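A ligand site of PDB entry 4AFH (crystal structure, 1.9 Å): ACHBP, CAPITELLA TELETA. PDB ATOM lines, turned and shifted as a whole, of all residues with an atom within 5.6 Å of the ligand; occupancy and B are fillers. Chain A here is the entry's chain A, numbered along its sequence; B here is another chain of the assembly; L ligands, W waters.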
ATOM      1  N   LYS A 100     -30.284 -20.514  -2.862  1.00  0.00           N
ATOM      2  CA  LYS A 100     -29.320 -21.579  -3.102  1.00  0.00           C
ATOM      3  C   LYS A 100     -28.666 -22.048  -1.802  1.00  0.00           C
ATOM      4  O   LYS A 100     -28.639 -21.306  -0.800  1.00  0.00           O
ATOM      5  CB  LYS A 100     -28.228 -21.082  -4.075  1.00  0.00           C
ATOM      6  CG  LYS A 100     -28.806 -20.555  -5.427  1.00  0.00           C
ATOM      7  CD  LYS A 100     -27.685 -20.242  -6.436  1.00  0.00           C
ATOM      8  CE  LYS A 100     -28.189 -20.356  -7.846  1.00  0.00           C
ATOM      9  NZ  LYS A 100     -28.292 -21.802  -8.191  1.00  0.00           N
ATOM     10  N   PHE A 102     -25.489 -22.263  -0.352  1.00  0.00           N
ATOM     11  CA  PHE A 102     -24.256 -21.532  -0.629  1.00  0.00           C
ATOM     12  C   PHE A 102     -23.044 -22.436  -0.438  1.00  0.00           C
ATOM     13  O   PHE A 102     -22.072 -22.381  -1.218  1.00  0.00           O
ATOM     14  CB  PHE A 102     -24.184 -20.323   0.333  1.00  0.00           C
ATOM     15  CG  PHE A 102     -22.873 -19.560   0.313  1.00  0.00           C
ATOM     16  CD1 PHE A 102     -22.434 -18.907  -0.837  1.00  0.00           C
ATOM     17  CD2 PHE A 102     -22.135 -19.435   1.470  1.00  0.00           C
ATOM     18  CE1 PHE A 102     -21.253 -18.171  -0.823  1.00  0.00           C
ATOM     19  CE2 PHE A 102     -20.947 -18.706   1.489  1.00  0.00           C
ATOM     20  CZ  PHE A 102     -20.507 -18.074   0.334  1.00  0.00           C
ATOM     21  N   GLN A 149     -26.190 -23.573   4.574  1.00  0.00           N
ATOM     22  CA  GLN A 149     -26.426 -22.128   4.479  1.00  0.00           C
ATOM     23  C   GLN A 149     -27.272 -21.798   3.247  1.00  0.00           C
ATOM     24  O   GLN A 149     -26.836 -22.048   2.104  1.00  0.00           O
ATOM     25  CB  GLN A 149     -25.089 -21.395   4.360  1.00  0.00           C
ATOM     26  CG  GLN A 149     -24.211 -21.540   5.575  1.00  0.00           C
ATOM     27  CD  GLN A 149     -22.805 -21.046   5.312  1.00  0.00           C
ATOM     28  OE1 GLN A 149     -21.903 -21.849   5.079  1.00  0.00           O
ATOM     29  NE2 GLN A 149     -22.620 -19.726   5.350  1.00  0.00           N
ATOM     30  N   PHE A 150     -28.450 -21.255   3.468  1.00  0.00           N
ATOM     31  CA  PHE A 150     -29.361 -20.913   2.364  1.00  0.00           C
ATOM     32  C   PHE A 150     -29.562 -19.422   2.276  1.00  0.00           C
ATOM     33  O   PHE A 150     -29.668 -18.738   3.284  1.00  0.00           O
ATOM     34  CB  PHE A 150     -30.725 -21.542   2.588  1.00  0.00           C
ATOM     35  CG  PHE A 150     -30.692 -23.036   2.689  1.00  0.00           C
ATOM     36  CD1 PHE A 150     -30.723 -23.824   1.549  1.00  0.00           C
ATOM     37  CD2 PHE A 150     -30.679 -23.652   3.933  1.00  0.00           C
ATOM     38  CE1 PHE A 150     -30.740 -25.199   1.646  1.00  0.00           C
ATOM     39  CE2 PHE A 150     -30.684 -25.016   4.045  1.00  0.00           C
ATOM     40  CZ  PHE A 150     -30.722 -25.806   2.912  1.00  0.00           C
ATOM     41  N   GLY A 151     -29.632 -18.887   1.054  1.00  0.00           N
ATOM     42  CA  GLY A 151     -29.978 -17.494   0.887  1.00  0.00           C
ATOM     43  C   GLY A 151     -30.219 -17.206  -0.574  1.00  0.00           C
ATOM     44  O   GLY A 151     -29.827 -18.008  -1.430  1.00  0.00           O
ATOM     45  N   SER A 152     -30.868 -16.082  -0.860  1.00  0.00           N
ATOM     46  CA  SER A 152     -31.008 -15.618  -2.223  1.00  0.00           C
ATOM     47  C   SER A 152     -29.635 -15.283  -2.820  1.00  0.00           C
ATOM     48  O   SER A 152     -28.802 -14.602  -2.195  1.00  0.00           O
ATOM     49  CB  SER A 152     -31.885 -14.356  -2.279  1.00  0.00           C
ATOM     50  OG  SER A 152     -31.765 -13.748  -3.560  1.00  0.00           O
ATOM     51  N   TRP A 153     -29.401 -15.743  -4.031  1.00  0.00           N
ATOM     52  CA  TRP A 153     -28.101 -15.479  -4.652  1.00  0.00           C
ATOM     53  C   TRP A 153     -27.881 -14.006  -4.967  1.00  0.00           C
ATOM     54  O   TRP A 153     -26.803 -13.458  -4.684  1.00  0.00           O
ATOM     55  CB  TRP A 153     -27.895 -16.299  -5.922  1.00  0.00           C
ATOM     56  CG  TRP A 153     -26.428 -16.412  -6.232  1.00  0.00           C
ATOM     57  CD1 TRP A 153     -25.705 -15.737  -7.177  1.00  0.00           C
ATOM     58  CD2 TRP A 153     -25.494 -17.235  -5.525  1.00  0.00           C
ATOM     59  NE1 TRP A 153     -24.386 -16.130  -7.129  1.00  0.00           N
ATOM     60  CE2 TRP A 153     -24.233 -17.048  -6.121  1.00  0.00           C
ATOM     61  CE3 TRP A 153     -25.614 -18.146  -4.465  1.00  0.00           C
ATOM     62  CZ2 TRP A 153     -23.085 -17.711  -5.677  1.00  0.00           C
ATOM     63  CZ3 TRP A 153     -24.482 -18.814  -4.024  1.00  0.00           C
ATOM     64  CH2 TRP A 153     -23.237 -18.595  -4.643  1.00  0.00           C
ATOM     65  N   VAL A 154     -28.884 -13.355  -5.543  1.00  0.00           N
ATOM     66  CA  VAL A 154     -28.669 -11.987  -5.981  1.00  0.00           C
ATOM     67  C   VAL A 154     -29.473 -10.926  -5.241  1.00  0.00           C
ATOM     68  O   VAL A 154     -29.142  -9.750  -5.341  1.00  0.00           O
ATOM     69  CB  VAL A 154     -28.882 -11.794  -7.500  1.00  0.00           C
ATOM     70  CG1 VAL A 154     -28.002 -12.777  -8.286  1.00  0.00           C
ATOM     71  CG2 VAL A 154     -30.353 -11.938  -7.865  1.00  0.00           C
ATOM     72  N   VAL A 192     -26.424 -10.993   6.531  1.00  0.00           N
ATOM     73  CA  VAL A 192     -24.980 -11.052   6.361  1.00  0.00           C
ATOM     74  C   VAL A 192     -24.491 -10.143   5.247  1.00  0.00           C
ATOM     75  O   VAL A 192     -25.004 -10.184   4.132  1.00  0.00           O
ATOM     76  CB  VAL A 192     -24.503 -12.486   6.044  1.00  0.00           C
ATOM     77  CG1 VAL A 192     -22.985 -12.533   5.911  1.00  0.00           C
ATOM     78  CG2 VAL A 192     -24.987 -13.446   7.118  1.00  0.00           C
ATOM     79  N   TYR A 194     -22.104  -8.992   2.354  1.00  0.00           N
ATOM     80  CA  TYR A 194     -21.171  -9.543   1.405  1.00  0.00           C
ATOM     81  C   TYR A 194     -20.364  -8.411   0.742  1.00  0.00           C
ATOM     82  O   TYR A 194     -20.831  -7.263   0.673  1.00  0.00           O
ATOM     83  CB  TYR A 194     -21.921 -10.432   0.390  1.00  0.00           C
ATOM     84  CG  TYR A 194     -22.184 -11.820   0.922  1.00  0.00           C
ATOM     85  CD1 TYR A 194     -23.187 -12.051   1.857  1.00  0.00           C
ATOM     86  CD2 TYR A 194     -21.409 -12.901   0.517  1.00  0.00           C
ATOM     87  CE1 TYR A 194     -23.428 -13.315   2.357  1.00  0.00           C
ATOM     88  CE2 TYR A 194     -21.643 -14.164   1.011  1.00  0.00           C
ATOM     89  CZ  TYR A 194     -22.646 -14.365   1.939  1.00  0.00           C
ATOM     90  OH  TYR A 194     -22.886 -15.622   2.428  1.00  0.00           O
ATOM     91  N   CYS A 196     -19.671  -7.777  -2.279  1.00  0.00           N
ATOM     92  CA  CYS A 196     -20.290  -7.260  -3.498  1.00  0.00           C
ATOM     93  C   CYS A 196     -21.174  -6.042  -3.232  1.00  0.00           C
ATOM     94  O   CYS A 196     -21.275  -5.138  -4.052  1.00  0.00           O
ATOM     95  CB  CYS A 196     -21.144  -8.344  -4.156  1.00  0.00           C
ATOM     96  SG  CYS A 196     -22.744  -8.681  -3.325  1.00  0.00           S
ATOM     97  N   CYS A 197     -21.822  -6.019  -2.067  1.00  0.00           N
ATOM     98  CA  CYS A 197     -23.032  -5.228  -1.928  1.00  0.00           C
ATOM     99  C   CYS A 197     -23.225  -4.492  -0.610  1.00  0.00           C
ATOM    100  O   CYS A 197     -22.827  -4.953   0.463  1.00  0.00           O
ATOM    101  CB  CYS A 197     -24.258  -6.124  -2.186  1.00  0.00           C
ATOM    102  SG  CYS A 197     -24.106  -7.173  -3.668  1.00  0.00           S
ATOM    103  N   TYR A 201     -27.516  -9.718   2.929  1.00  0.00           N
ATOM    104  CA  TYR A 201     -28.255 -10.870   2.435  1.00  0.00           C
ATOM    105  C   TYR A 201     -28.746 -11.677   3.620  1.00  0.00           C
ATOM    106  O   TYR A 201     -28.030 -11.824   4.615  1.00  0.00           O
ATOM    107  CB  TYR A 201     -27.360 -11.725   1.537  1.00  0.00           C
ATOM    108  CG  TYR A 201     -27.141 -11.104   0.186  1.00  0.00           C
ATOM    109  CD1 TYR A 201     -26.193 -10.098   0.011  1.00  0.00           C
ATOM    110  CD2 TYR A 201     -27.891 -11.495  -0.896  1.00  0.00           C
ATOM    111  CE1 TYR A 201     -26.002  -9.513  -1.231  1.00  0.00           C
ATOM    112  CE2 TYR A 201     -27.716 -10.915  -2.141  1.00  0.00           C
ATOM    113  CZ  TYR A 201     -26.775  -9.940  -2.302  1.00  0.00           C
ATOM    114  OH  TYR A 201     -26.610  -9.370  -3.546  1.00  0.00           O
ATOM    115  N   VAL A 202     -29.958 -12.194   3.531  1.00  0.00           N
ATOM    116  CA  VAL A 202     -30.524 -13.000   4.620  1.00  0.00           C
ATOM    117  C   VAL A 202     -29.985 -14.415   4.511  1.00  0.00           C
ATOM    118  O   VAL A 202     -30.134 -15.052   3.465  1.00  0.00           O
ATOM    119  CB  VAL A 202     -32.057 -13.047   4.561  1.00  0.00           C
ATOM    120  CG1 VAL A 202     -32.618 -13.837   5.736  1.00  0.00           C
ATOM    121  CG2 VAL A 202     -32.627 -11.613   4.539  1.00  0.00           C
ATOM    122  N   GLU A 203     -29.349 -14.913   5.558  1.00  0.00           N
ATOM    123  CA  GLU A 203     -28.872 -16.293   5.541  1.00  0.00           C
ATOM    124  C   GLU A 203     -29.661 -17.125   6.534  1.00  0.00           C
ATOM    125  O   GLU A 203     -29.748 -16.743   7.715  1.00  0.00           O
ATOM    126  CB  GLU A 203     -27.418 -16.345   5.951  1.00  0.00           C
ATOM    127  CG  GLU A 203     -26.953 -17.762   6.268  1.00  0.00           C
ATOM    128  CD  GLU A 203     -25.555 -17.784   6.851  1.00  0.00           C
ATOM    129  OE1 GLU A 203     -25.391 -17.457   8.047  1.00  0.00           O
ATOM    130  OE2 GLU A 203     -24.624 -18.085   6.091  1.00  0.00           O
ATOM    131  N   MET A 204     -30.199 -18.259   6.081  1.00  0.00           N
ATOM    132  CA  MET A 204     -30.786 -19.256   6.959  1.00  0.00           C
ATOM    133  C   MET A 204     -29.725 -20.341   7.144  1.00  0.00           C
ATOM    134  O   MET A 204     -29.402 -21.060   6.194  1.00  0.00           O
ATOM    135  CB  MET A 204     -32.039 -19.877   6.303  1.00  0.00           C
ATOM    136  CG  MET A 204     -33.019 -18.845   5.756  1.00  0.00           C
ATOM    137  SD  MET A 204     -33.500 -17.654   7.030  1.00  0.00           S
ATOM    138  CE  MET A 204     -34.967 -18.425   7.701  1.00  0.00           C
ATOM    139  N   ILE B  64     -16.422 -19.973  -6.466  1.00  0.00           N
ATOM    140  CA  ILE B  64     -17.338 -18.983  -7.002  1.00  0.00           C
ATOM    141  C   ILE B  64     -16.540 -18.119  -7.991  1.00  0.00           C
ATOM    142  O   ILE B  64     -15.469 -17.632  -7.688  1.00  0.00           O
ATOM    143  CB  ILE B  64     -17.970 -18.164  -5.876  1.00  0.00           C
ATOM    144  CG1 ILE B  64     -18.885 -19.082  -5.029  1.00  0.00           C
ATOM    145  CG2 ILE B  64     -18.757 -17.006  -6.450  1.00  0.00           C
ATOM    146  CD1 ILE B  64     -19.508 -18.400  -3.829  1.00  0.00           C
ATOM    147  N   THR B 115     -27.942 -19.006 -12.351  1.00  0.00           N
ATOM    148  CA  THR B 115     -27.619 -17.818 -11.544  1.00  0.00           C
ATOM    149  C   THR B 115     -27.836 -16.528 -12.350  1.00  0.00           C
ATOM    150  O   THR B 115     -27.323 -16.418 -13.458  1.00  0.00           O
ATOM    151  CB  THR B 115     -26.134 -17.876 -11.103  1.00  0.00           C
ATOM    152  OG1 THR B 115     -25.964 -18.935 -10.133  1.00  0.00           O
ATOM    153  CG2 THR B 115     -25.690 -16.576 -10.494  1.00  0.00           C
ATOM    154  N   GLN B 116     -28.551 -15.554 -11.808  1.00  0.00           N
ATOM    155  CA  GLN B 116     -28.793 -14.343 -12.572  1.00  0.00           C
ATOM    156  C   GLN B 116     -27.596 -13.406 -12.574  1.00  0.00           C
ATOM    157  O   GLN B 116     -26.797 -13.384 -11.635  1.00  0.00           O
ATOM    158  CB  GLN B 116     -30.043 -13.626 -12.065  1.00  0.00           C
ATOM    159  CG  GLN B 116     -31.304 -14.421 -12.271  1.00  0.00           C
ATOM    160  CD  GLN B 116     -32.482 -13.764 -11.613  1.00  0.00           C
ATOM    161  OE1 GLN B 116     -32.612 -13.782 -10.383  1.00  0.00           O
ATOM    162  NE2 GLN B 116     -33.351 -13.159 -12.418  1.00  0.00           N
ATOM    163  N   ALA B 117     -27.456 -12.658 -13.660  1.00  0.00           N
ATOM    164  CA  ALA B 117     -26.450 -11.613 -13.790  1.00  0.00           C
ATOM    165  C   ALA B 117     -27.148 -10.284 -13.502  1.00  0.00           C
ATOM    166  O   ALA B 117     -28.347 -10.153 -13.705  1.00  0.00           O
ATOM    167  CB  ALA B 117     -25.881 -11.616 -15.214  1.00  0.00           C
ATOM    168  N   ILE B 118     -26.411  -9.301 -13.013  1.00  0.00           N
ATOM    169  CA  ILE B 118     -26.966  -7.963 -12.852  1.00  0.00           C
ATOM    170  C   ILE B 118     -26.352  -7.041 -13.916  1.00  0.00           C
ATOM    171  O   ILE B 118     -25.137  -7.039 -14.122  1.00  0.00           O
ATOM    172  CB  ILE B 118     -26.691  -7.413 -11.428  1.00  0.00           C
ATOM    173  CG1 ILE B 118     -27.355  -8.305 -10.348  1.00  0.00           C
ATOM    174  CG2 ILE B 118     -27.096  -5.940 -11.306  1.00  0.00           C
ATOM    175  CD1 ILE B 118     -28.813  -8.575 -10.540  1.00  0.00           C
ATOM    176  N   PHE B 120     -26.056  -3.032 -15.112  1.00  0.00           N
ATOM    177  CA  PHE B 120     -26.243  -1.657 -14.680  1.00  0.00           C
ATOM    178  C   PHE B 120     -26.571  -0.797 -15.892  1.00  0.00           C
ATOM    179  O   PHE B 120     -26.348  -1.236 -17.033  1.00  0.00           O
ATOM    180  CB  PHE B 120     -24.980  -1.158 -13.974  1.00  0.00           C
ATOM    181  CG  PHE B 120     -24.722  -1.846 -12.668  1.00  0.00           C
ATOM    182  CD1 PHE B 120     -24.014  -3.044 -12.625  1.00  0.00           C
ATOM    183  CD2 PHE B 120     -25.188  -1.311 -11.492  1.00  0.00           C
ATOM    184  CE1 PHE B 120     -23.784  -3.689 -11.427  1.00  0.00           C
ATOM    185  CE2 PHE B 120     -24.961  -1.942 -10.277  1.00  0.00           C
ATOM    186  CZ  PHE B 120     -24.259  -3.135 -10.239  1.00  0.00           C
ATOM    187  N   LEU B 126     -22.422  -7.695 -14.190  1.00  0.00           N
ATOM    188  CA  LEU B 126     -21.700  -8.397 -13.138  1.00  0.00           C
ATOM    189  C   LEU B 126     -22.388  -9.727 -12.882  1.00  0.00           C
ATOM    190  O   LEU B 126     -23.571  -9.771 -12.550  1.00  0.00           O
ATOM    191  CB  LEU B 126     -21.657  -7.560 -11.851  1.00  0.00           C
ATOM    192  CG  LEU B 126     -20.938  -8.122 -10.612  1.00  0.00           C
ATOM    193  CD1 LEU B 126     -19.505  -8.560 -10.918  1.00  0.00           C
ATOM    194  CD2 LEU B 126     -20.981  -7.112  -9.473  1.00  0.00           C
ATOM    195  N   TRP B 127     -21.633 -10.812 -13.040  1.00  0.00           N
ATOM    196  CA  TRP B 127     -22.224 -12.140 -12.933  1.00  0.00           C
ATOM    197  C   TRP B 127     -21.300 -13.023 -12.089  1.00  0.00           C
ATOM    198  O   TRP B 127     -20.098 -13.098 -12.360  1.00  0.00           O
ATOM    199  CB  TRP B 127     -22.461 -12.722 -14.326  1.00  0.00           C
ATOM    200  CG  TRP B 127     -23.070 -14.078 -14.321  1.00  0.00           C
ATOM    201  CD1 TRP B 127     -24.074 -14.544 -13.499  1.00  0.00           C
ATOM    202  CD2 TRP B 127     -22.709 -15.188 -15.178  1.00  0.00           C
ATOM    203  NE1 TRP B 127     -24.365 -15.858 -13.798  1.00  0.00           N
ATOM    204  CE2 TRP B 127     -23.552 -16.282 -14.826  1.00  0.00           C
ATOM    205  CE3 TRP B 127     -21.800 -15.351 -16.221  1.00  0.00           C
ATOM    206  CZ2 TRP B 127     -23.480 -17.514 -15.460  1.00  0.00           C
ATOM    207  CZ3 TRP B 127     -21.712 -16.579 -16.851  1.00  0.00           C
ATOM    208  CH2 TRP B 127     -22.560 -17.652 -16.470  1.00  0.00           C
ATOM    209  N   ILE B 128     -21.845 -13.647 -11.044  1.00  0.00           N
ATOM    210  CA  ILE B 128     -21.018 -14.328 -10.023  1.00  0.00           C
ATOM    211  C   ILE B 128     -21.536 -15.744  -9.758  1.00  0.00           C
ATOM    212  O   ILE B 128     -22.077 -16.030  -8.687  1.00  0.00           O
ATOM    213  CB  ILE B 128     -20.959 -13.465  -8.726  1.00  0.00           C
ATOM    214  CG1 ILE B 128     -20.476 -12.045  -9.057  1.00  0.00           C
ATOM    215  CG2 ILE B 128     -20.053 -14.065  -7.641  1.00  0.00           C
ATOM    216  CD1 ILE B 128     -20.582 -11.089  -7.896  1.00  0.00           C
ATOM    217  N   PHE B 175     -14.522 -16.247   0.419  1.00  0.00           N
ATOM    218  CA  PHE B 175     -15.553 -17.261   0.667  1.00  0.00           C
ATOM    219  C   PHE B 175     -14.984 -18.597   1.150  1.00  0.00           C
ATOM    220  O   PHE B 175     -15.684 -19.603   1.157  1.00  0.00           O
ATOM    221  CB  PHE B 175     -16.365 -17.510  -0.604  1.00  0.00           C
ATOM    222  CG  PHE B 175     -17.103 -16.301  -1.110  1.00  0.00           C
ATOM    223  CD1 PHE B 175     -17.758 -15.447  -0.239  1.00  0.00           C
ATOM    224  CD2 PHE B 175     -17.152 -16.025  -2.458  1.00  0.00           C
ATOM    225  CE1 PHE B 175     -18.445 -14.334  -0.717  1.00  0.00           C
ATOM    226  CE2 PHE B 175     -17.847 -14.915  -2.947  1.00  0.00           C
ATOM    227  CZ  PHE B 175     -18.492 -14.073  -2.083  1.00  0.00           C
HETATM  228  O1  LIG L   1     -24.294 -12.631  -7.404  1.00  0.00           O
HETATM  229  C1  LIG L   1     -24.330 -11.667  -6.659  1.00  0.00           C
HETATM  230  C2  LIG L   1     -26.563 -16.962   2.432  1.00  0.00           C
HETATM  231  C3  LIG L   1     -26.422 -15.598   2.212  1.00  0.00           C
HETATM  232  C4  LIG L   1     -26.147 -15.122   0.924  1.00  0.00           C
HETATM  233  C5  LIG L   1     -25.991 -16.012  -0.134  1.00  0.00           C
HETATM  234  C6  LIG L   1     -26.126 -17.382   0.091  1.00  0.00           C
HETATM  235  C7  LIG L   1     -26.420 -17.870   1.370  1.00  0.00           C
HETATM  236  C8  LIG L   1     -24.166 -15.341  -1.585  1.00  0.00           C
HETATM  237  C9  LIG L   1     -23.642 -14.886  -2.970  1.00  0.00           C
HETATM  238  C10 LIG L   1     -22.104 -14.919  -3.018  1.00  0.00           C
HETATM  239  C11 LIG L   1     -21.629 -14.558  -4.423  1.00  0.00           C
HETATM  240  C12 LIG L   1     -22.173 -13.193  -4.811  1.00  0.00           C
HETATM  241  C13 LIG L   1     -23.705 -13.202  -4.738  1.00  0.00           C
HETATM  242  N1  LIG L   1     -24.183 -13.557  -3.380  1.00  0.00           N
HETATM  243  C14 LIG L   1     -23.856 -12.498  -2.412  1.00  0.00           C
HETATM  244  C15 LIG L   1     -24.245 -11.814  -5.145  1.00  0.00           C
HETATM  245  C16 LIG L   1     -25.673 -15.512  -1.503  1.00  0.00           C
HETATM  246  O2  LIG L   1     -26.300 -14.248  -1.710  1.00  0.00           O
HETATM  247  C17 LIG L   1     -24.778  -9.192  -6.461  1.00  0.00           C
HETATM  248  C18 LIG L   1     -24.436 -10.286  -7.259  1.00  0.00           C
HETATM  249  C19 LIG L   1     -24.196 -10.107  -8.624  1.00  0.00           C
HETATM  250  C20 LIG L   1     -24.289  -8.832  -9.181  1.00  0.00           C
HETATM  251  C21 LIG L   1     -24.627  -7.752  -8.383  1.00  0.00           C
HETATM  252  C22 LIG L   1     -24.864  -7.916  -7.025  1.00  0.00           C
HETATM  253  O   HOH W   1     -24.575 -13.405 -10.034  1.00  0.00           O
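The backbone carbonyl oxygen (O) of Ile 118 of chain B lies within hydrogen-bond range of the backbone NH (N) of Leu 126 of chain B (2.8 Å).
NE1 of Trp 153 lies within hydrogen-bond range of O of Ile 128 of chain B, at 2.8 Å.
OH of Tyr 201 lies within hydrogen-bond range of O of Val 154 (3.1 Å).
The side-chain sulfur (SG) of Cys 197 sits at hydrogen-bond distance from the side-chain hydroxyl (OH) of Tyr 201.
The backbone NH (N) of Phe 102 lies within hydrogen-bond range of the backbone carbonyl oxygen (O) of Gln 149 (2.8 Å).
The backbone NH (N) of Val 192 sits at hydrogen-bond distance from the backbone carbonyl oxygen (O) of Tyr 201, 2.6 Å away.
N of Met 204 sits at hydrogen-bond distance from O of Phe 150 (2.9 Å).
The side-chain carboxylate (OE2) of Glu 203 sits at hydrogen-bond distance from the side-chain amide nitrogen (NE2) of Gln 149 (2.7 Å).
O of Trp 153 sits close to O2 of the ligand (3.1 Å).
The backbone carbonyl oxygen of Ser 152 lies within hydrogen-bond range of an oxygen (O2) of the ligand (2.6 Å).
Residues that only touch the ligand: Phe 102, Phe 150, Gly 151, Val 154, Tyr 194, Cys 196, Cys 197, Tyr 201, Val 202, Glu 203, Ile 118 of chain B, Leu 126 of chain B, Ile 128 of chain B and Phe 175 of chain B.
Hydrophobic or aromatic side chains within 4 Å of the ligand: Phe 102, Trp 153, Val 154, Tyr 194, Tyr 201, Ile 118 of chain B, Leu 126 of chain B, Ile 128 of chain B and Phe 175 of chain B.
Water W1 lies within hydrogen-bond range of the backbone carbonyl oxygen of Gln 116 of chain B, an oxygen (O1) of the ligand and the backbone NH of Ile 128 of chain B.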
